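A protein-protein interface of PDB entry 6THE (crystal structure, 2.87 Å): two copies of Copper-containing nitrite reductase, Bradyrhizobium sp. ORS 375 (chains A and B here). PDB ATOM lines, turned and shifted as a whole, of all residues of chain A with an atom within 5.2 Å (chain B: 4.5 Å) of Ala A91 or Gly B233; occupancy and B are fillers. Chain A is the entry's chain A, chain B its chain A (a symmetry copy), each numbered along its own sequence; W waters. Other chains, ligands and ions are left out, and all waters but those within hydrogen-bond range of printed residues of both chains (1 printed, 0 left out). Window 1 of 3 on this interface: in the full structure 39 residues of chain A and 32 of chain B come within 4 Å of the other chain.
The backbone carbonyl oxygen (O) of Gly B233 lies within hydrogen-bond range of the backbone NH (N) of Ala A93 (3.2 Å).
The backbone carbonyl oxygen (O) of Ala A91 lies close to the backbone carbonyl oxygen (O) of Gly B233 (3.4 Å).
Ile B232 touches Asp A87 (CG2 to OD2, 3.5 Å).
His A89 touches Ile B235 (O to CG1, 3.2 Å).
Ile B235 touches Ala A90.
Gly B233 touches Ile A92 (O to CA, 3.3 Å).
Ile A92 touches Glu B234 (CG2 to OE2, 3.6 Å).
N of Ile B235 touches CD1 of Ile A92, 3.7 Å away.
Tyr B276 touches Ala A93.
CA of Gly A95 touches CG2 of Ile B232 (3.6 Å).
CA of Gly B233 touches N of Gly A96, at 3.7 Å.
No position is printed for both chains.
Of the 11 pairs that touch across the chains among the printed residues, none has its exchanged pair printed and touching as well.
Hydrophobic or aromatic side chains of chain A within 4 Å of the printed part of chain B: Ile A92.
Among the printed residues, 11 pairs touch across the chains.
Of chain A, only Ala A91, Ile A92, Ala A93 and Gly A96 come within 4 Å of Gly B233.
Of the printed residues of chain B, His A89 touches Ile B235 (3.2 Å).
Of the printed residues of chain A, Glu B234 touches Ile A92.
Trp A113 touches none of the printed residues of chain B.
Pro A94 touches none of the printed residues of chain B.
The nearest printed residue of chain B that does not touch Gly A95 is Gly B233 (4.4 Å).
N of Phe A88 is in hydrogen-bond range of O of Gly A96.
Water W1 bridges the side-chain carboxylate (OD1) of Asp A87 and the backbone NH (N) of Gly B233.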
ATOM      1  N   ASP A  87      15.809  21.212 -14.749  1.00  0.00           N
ATOM      2  CA  ASP A  87      14.990  21.853 -15.763  1.00  0.00           C
ATOM      3  C   ASP A  87      15.654  21.654 -17.122  1.00  0.00           C
ATOM      4  O   ASP A  87      16.748  22.161 -17.360  1.00  0.00           O
ATOM      5  CB  ASP A  87      14.774  23.334 -15.422  1.00  0.00           C
ATOM      6  CG  ASP A  87      14.146  24.175 -16.524  1.00  0.00           C
ATOM      7  OD1 ASP A  87      13.677  23.596 -17.526  1.00  0.00           O
ATOM      8  OD2 ASP A  87      14.129  25.412 -16.369  1.00  0.00           O
ATOM      9  N   PHE A  88      14.973  20.912 -18.003  1.00  0.00           N
ATOM     10  CA  PHE A  88      15.460  20.660 -19.349  1.00  0.00           C
ATOM     11  C   PHE A  88      14.843  21.672 -20.310  1.00  0.00           C
ATOM     12  O   PHE A  88      13.630  21.876 -20.312  1.00  0.00           O
ATOM     13  CB  PHE A  88      15.146  19.224 -19.781  1.00  0.00           C
ATOM     14  CG  PHE A  88      15.776  18.148 -18.934  1.00  0.00           C
ATOM     15  CD1 PHE A  88      17.080  17.731 -19.165  1.00  0.00           C
ATOM     16  CD2 PHE A  88      15.064  17.541 -17.909  1.00  0.00           C
ATOM     17  CE1 PHE A  88      17.658  16.739 -18.387  1.00  0.00           C
ATOM     18  CE2 PHE A  88      15.643  16.548 -17.132  1.00  0.00           C
ATOM     19  CZ  PHE A  88      16.938  16.148 -17.372  1.00  0.00           C
ATOM     20  N   HIS A  89      15.700  22.298 -21.126  1.00  0.00           N
ATOM     21  CA  HIS A  89      15.269  23.260 -22.128  1.00  0.00           C
ATOM     22  C   HIS A  89      14.749  22.528 -23.363  1.00  0.00           C
ATOM     23  O   HIS A  89      14.145  23.142 -24.240  1.00  0.00           O
ATOM     24  CB  HIS A  89      16.412  24.225 -22.473  1.00  0.00           C
ATOM     25  CG  HIS A  89      16.663  25.282 -21.449  1.00  0.00           C
ATOM     26  ND1 HIS A  89      17.024  26.568 -21.797  1.00  0.00           N
ATOM     27  CD2 HIS A  89      16.606  25.257 -20.100  1.00  0.00           C
ATOM     28  CE1 HIS A  89      17.188  27.288 -20.707  1.00  0.00           C
ATOM     29  NE2 HIS A  89      16.934  26.508 -19.650  1.00  0.00           N
ATOM     30  N   ALA A  90      14.994  21.214 -23.415  1.00  0.00           N
ATOM     31  CA  ALA A  90      14.555  20.374 -24.517  1.00  0.00           C
ATOM     32  C   ALA A  90      13.146  19.848 -24.249  1.00  0.00           C
ATOM     33  O   ALA A  90      12.531  19.244 -25.126  1.00  0.00           O
ATOM     34  CB  ALA A  90      15.534  19.243 -24.714  1.00  0.00           C
ATOM     35  N   ALA A  91      12.646  20.097 -23.032  1.00  0.00           N
ATOM     36  CA  ALA A  91      11.401  19.508 -22.564  1.00  0.00           C
ATOM     37  C   ALA A  91      10.247  20.497 -22.704  1.00  0.00           C
ATOM     38  O   ALA A  91      10.394  21.685 -22.420  1.00  0.00           O
ATOM     39  CB  ALA A  91      11.560  19.047 -21.135  1.00  0.00           C
ATOM     40  N   ILE A  92       9.098  19.975 -23.153  1.00  0.00           N
ATOM     41  CA  ILE A  92       7.835  20.694 -23.125  1.00  0.00           C
ATOM     42  C   ILE A  92       7.069  20.221 -21.890  1.00  0.00           C
ATOM     43  O   ILE A  92       6.264  19.294 -21.965  1.00  0.00           O
ATOM     44  CB  ILE A  92       7.038  20.480 -24.432  1.00  0.00           C
ATOM     45  CG1 ILE A  92       7.897  20.684 -25.687  1.00  0.00           C
ATOM     46  CG2 ILE A  92       5.776  21.333 -24.458  1.00  0.00           C
ATOM     47  CD1 ILE A  92       8.395  22.101 -25.895  1.00  0.00           C
ATOM     48  N   ALA A  93       7.358  20.862 -20.751  1.00  0.00           N
ATOM     49  CA  ALA A  93       6.830  20.461 -19.457  1.00  0.00           C
ATOM     50  C   ALA A  93       6.870  21.650 -18.501  1.00  0.00           C
ATOM     51  O   ALA A  93       7.761  22.490 -18.604  1.00  0.00           O
ATOM     52  CB  ALA A  93       7.641  19.308 -18.918  1.00  0.00           C
ATOM     53  N   PRO A  94       5.919  21.763 -17.540  1.00  0.00           N
ATOM     54  CA  PRO A  94       5.948  22.841 -16.550  1.00  0.00           C
ATOM     55  C   PRO A  94       7.255  22.821 -15.760  1.00  0.00           C
ATOM     56  O   PRO A  94       7.599  21.814 -15.144  1.00  0.00           O
ATOM     57  CB  PRO A  94       4.761  22.527 -15.627  1.00  0.00           C
ATOM     58  CG  PRO A  94       3.839  21.685 -16.479  1.00  0.00           C
ATOM     59  CD  PRO A  94       4.761  20.872 -17.363  1.00  0.00           C
ATOM     60  N   GLY A  95       7.983  23.943 -15.816  1.00  0.00           N
ATOM     61  CA  GLY A  95       9.272  24.077 -15.158  1.00  0.00           C
ATOM     62  C   GLY A  95      10.361  23.264 -15.857  1.00  0.00           C
ATOM     63  O   GLY A  95      11.438  23.065 -15.299  1.00  0.00           O
ATOM     64  N   GLY A  96      10.064  22.805 -17.080  1.00  0.00           N
ATOM     65  CA  GLY A  96      10.961  21.953 -17.841  1.00  0.00           C
ATOM     66  C   GLY A  96      11.059  20.552 -17.244  1.00  0.00           C
ATOM     67  O   GLY A  96      12.043  19.848 -17.462  1.00  0.00           O
ATOM     68  N   GLY A  97      10.023  20.166 -16.489  1.00  0.00           N
ATOM     69  CA  GLY A  97       9.956  18.867 -15.840  1.00  0.00           C
ATOM     70  C   GLY A  97      10.435  18.917 -14.390  1.00  0.00           C
ATOM     71  O   GLY A  97      10.463  17.893 -13.713  1.00  0.00           O
ATOM     72  N   TRP A 113       9.643  12.549 -20.586  1.00  0.00           N
ATOM     73  CA  TRP A 113       9.315  13.585 -21.553  1.00  0.00           C
ATOM     74  C   TRP A 113       9.861  13.199 -22.925  1.00  0.00           C
ATOM     75  O   TRP A 113      10.850  12.477 -23.023  1.00  0.00           O
ATOM     76  CB  TRP A 113       9.826  14.958 -21.092  1.00  0.00           C
ATOM     77  CG  TRP A 113      11.312  15.039 -20.908  1.00  0.00           C
ATOM     78  CD1 TRP A 113      12.014  14.752 -19.774  1.00  0.00           C
ATOM     79  CD2 TRP A 113      12.284  15.446 -21.889  1.00  0.00           C
ATOM     80  NE1 TRP A 113      13.353  14.946 -19.981  1.00  0.00           N
ATOM     81  CE2 TRP A 113      13.550  15.371 -21.268  1.00  0.00           C
ATOM     82  CE3 TRP A 113      12.213  15.859 -23.225  1.00  0.00           C
ATOM     83  CZ2 TRP A 113      14.730  15.697 -21.939  1.00  0.00           C
ATOM     84  CZ3 TRP A 113      13.380  16.181 -23.888  1.00  0.00           C
ATOM     85  CH2 TRP A 113      14.619  16.099 -23.251  1.00  0.00           C
ATOM     86  N   VAL B 231      10.867  31.186 -22.069  1.00  0.00           N
ATOM     87  CA  VAL B 231       9.684  30.688 -21.389  1.00  0.00           C
ATOM     88  C   VAL B 231      10.027  29.313 -20.820  1.00  0.00           C
ATOM     89  O   VAL B 231      10.326  28.386 -21.573  1.00  0.00           O
ATOM     90  CB  VAL B 231       8.457  30.638 -22.325  1.00  0.00           C
ATOM     91  CG1 VAL B 231       7.241  30.034 -21.640  1.00  0.00           C
ATOM     92  CG2 VAL B 231       8.120  32.009 -22.894  1.00  0.00           C
ATOM     93  N   ILE B 232       9.999  29.205 -19.487  1.00  0.00           N
ATOM     94  CA  ILE B 232      10.387  27.985 -18.797  1.00  0.00           C
ATOM     95  C   ILE B 232       9.337  26.911 -19.065  1.00  0.00           C
ATOM     96  O   ILE B 232       8.173  27.065 -18.697  1.00  0.00           O
ATOM     97  CB  ILE B 232      10.610  28.221 -17.288  1.00  0.00           C
ATOM     98  CG1 ILE B 232      11.633  29.331 -17.026  1.00  0.00           C
ATOM     99  CG2 ILE B 232      11.002  26.923 -16.596  1.00  0.00           C
ATOM    100  CD1 ILE B 232      11.931  29.576 -15.562  1.00  0.00           C
ATOM    101  N   GLY B 233       9.777  25.830 -19.718  1.00  0.00           N
ATOM    102  CA  GLY B 233       8.924  24.697 -20.029  1.00  0.00           C
ATOM    103  C   GLY B 233       8.504  24.670 -21.496  1.00  0.00           C
ATOM    104  O   GLY B 233       7.750  23.790 -21.908  1.00  0.00           O
ATOM    105  N   GLU B 234       9.005  25.634 -22.276  1.00  0.00           N
ATOM    106  CA  GLU B 234       8.627  25.765 -23.674  1.00  0.00           C
ATOM    107  C   GLU B 234       9.862  25.994 -24.543  1.00  0.00           C
ATOM    108  O   GLU B 234      10.868  26.529 -24.081  1.00  0.00           O
ATOM    109  CB  GLU B 234       7.614  26.897 -23.855  1.00  0.00           C
ATOM    110  CG  GLU B 234       6.180  26.488 -23.559  1.00  0.00           C
ATOM    111  CD  GLU B 234       5.567  25.470 -24.509  1.00  0.00           C
ATOM    112  OE1 GLU B 234       5.980  25.426 -25.688  1.00  0.00           O
ATOM    113  OE2 GLU B 234       4.673  24.720 -24.067  1.00  0.00           O
ATOM    114  N   ILE B 235       9.756  25.564 -25.806  1.00  0.00           N
ATOM    115  CA  ILE B 235      10.727  25.867 -26.844  1.00  0.00           C
ATOM    116  C   ILE B 235      10.018  26.698 -27.910  1.00  0.00           C
ATOM    117  O   ILE B 235       8.907  26.364 -28.320  1.00  0.00           O
ATOM    118  CB  ILE B 235      11.332  24.577 -27.440  1.00  0.00           C
ATOM    119  CG1 ILE B 235      11.815  23.610 -26.355  1.00  0.00           C
ATOM    120  CG2 ILE B 235      12.437  24.905 -28.435  1.00  0.00           C
ATOM    121  CD1 ILE B 235      12.090  22.207 -26.849  1.00  0.00           C
ATOM    122  N   TYR B 276       3.841  27.962 -16.560  1.00  0.00           N
ATOM    123  CA  TYR B 276       5.022  28.283 -17.344  1.00  0.00           C
ATOM    124  C   TYR B 276       5.519  29.671 -16.949  1.00  0.00           C
ATOM    125  O   TYR B 276       4.720  30.569 -16.690  1.00  0.00           O
ATOM    126  CB  TYR B 276       4.713  28.175 -18.839  1.00  0.00           C
ATOM    127  CG  TYR B 276       4.423  26.774 -19.320  1.00  0.00           C
ATOM    128  CD1 TYR B 276       3.160  26.215 -19.183  1.00  0.00           C
ATOM    129  CD2 TYR B 276       5.410  26.003 -19.912  1.00  0.00           C
ATOM    130  CE1 TYR B 276       2.888  24.928 -19.619  1.00  0.00           C
ATOM    131  CE2 TYR B 276       5.155  24.715 -20.354  1.00  0.00           C
ATOM    132  CZ  TYR B 276       3.888  24.175 -20.208  1.00  0.00           C
ATOM    133  OH  TYR B 276       3.632  22.908 -20.643  1.00  0.00           O
HETATM  134  O   HOH W   1      12.679  25.357 -19.384  1.00  0.00           O
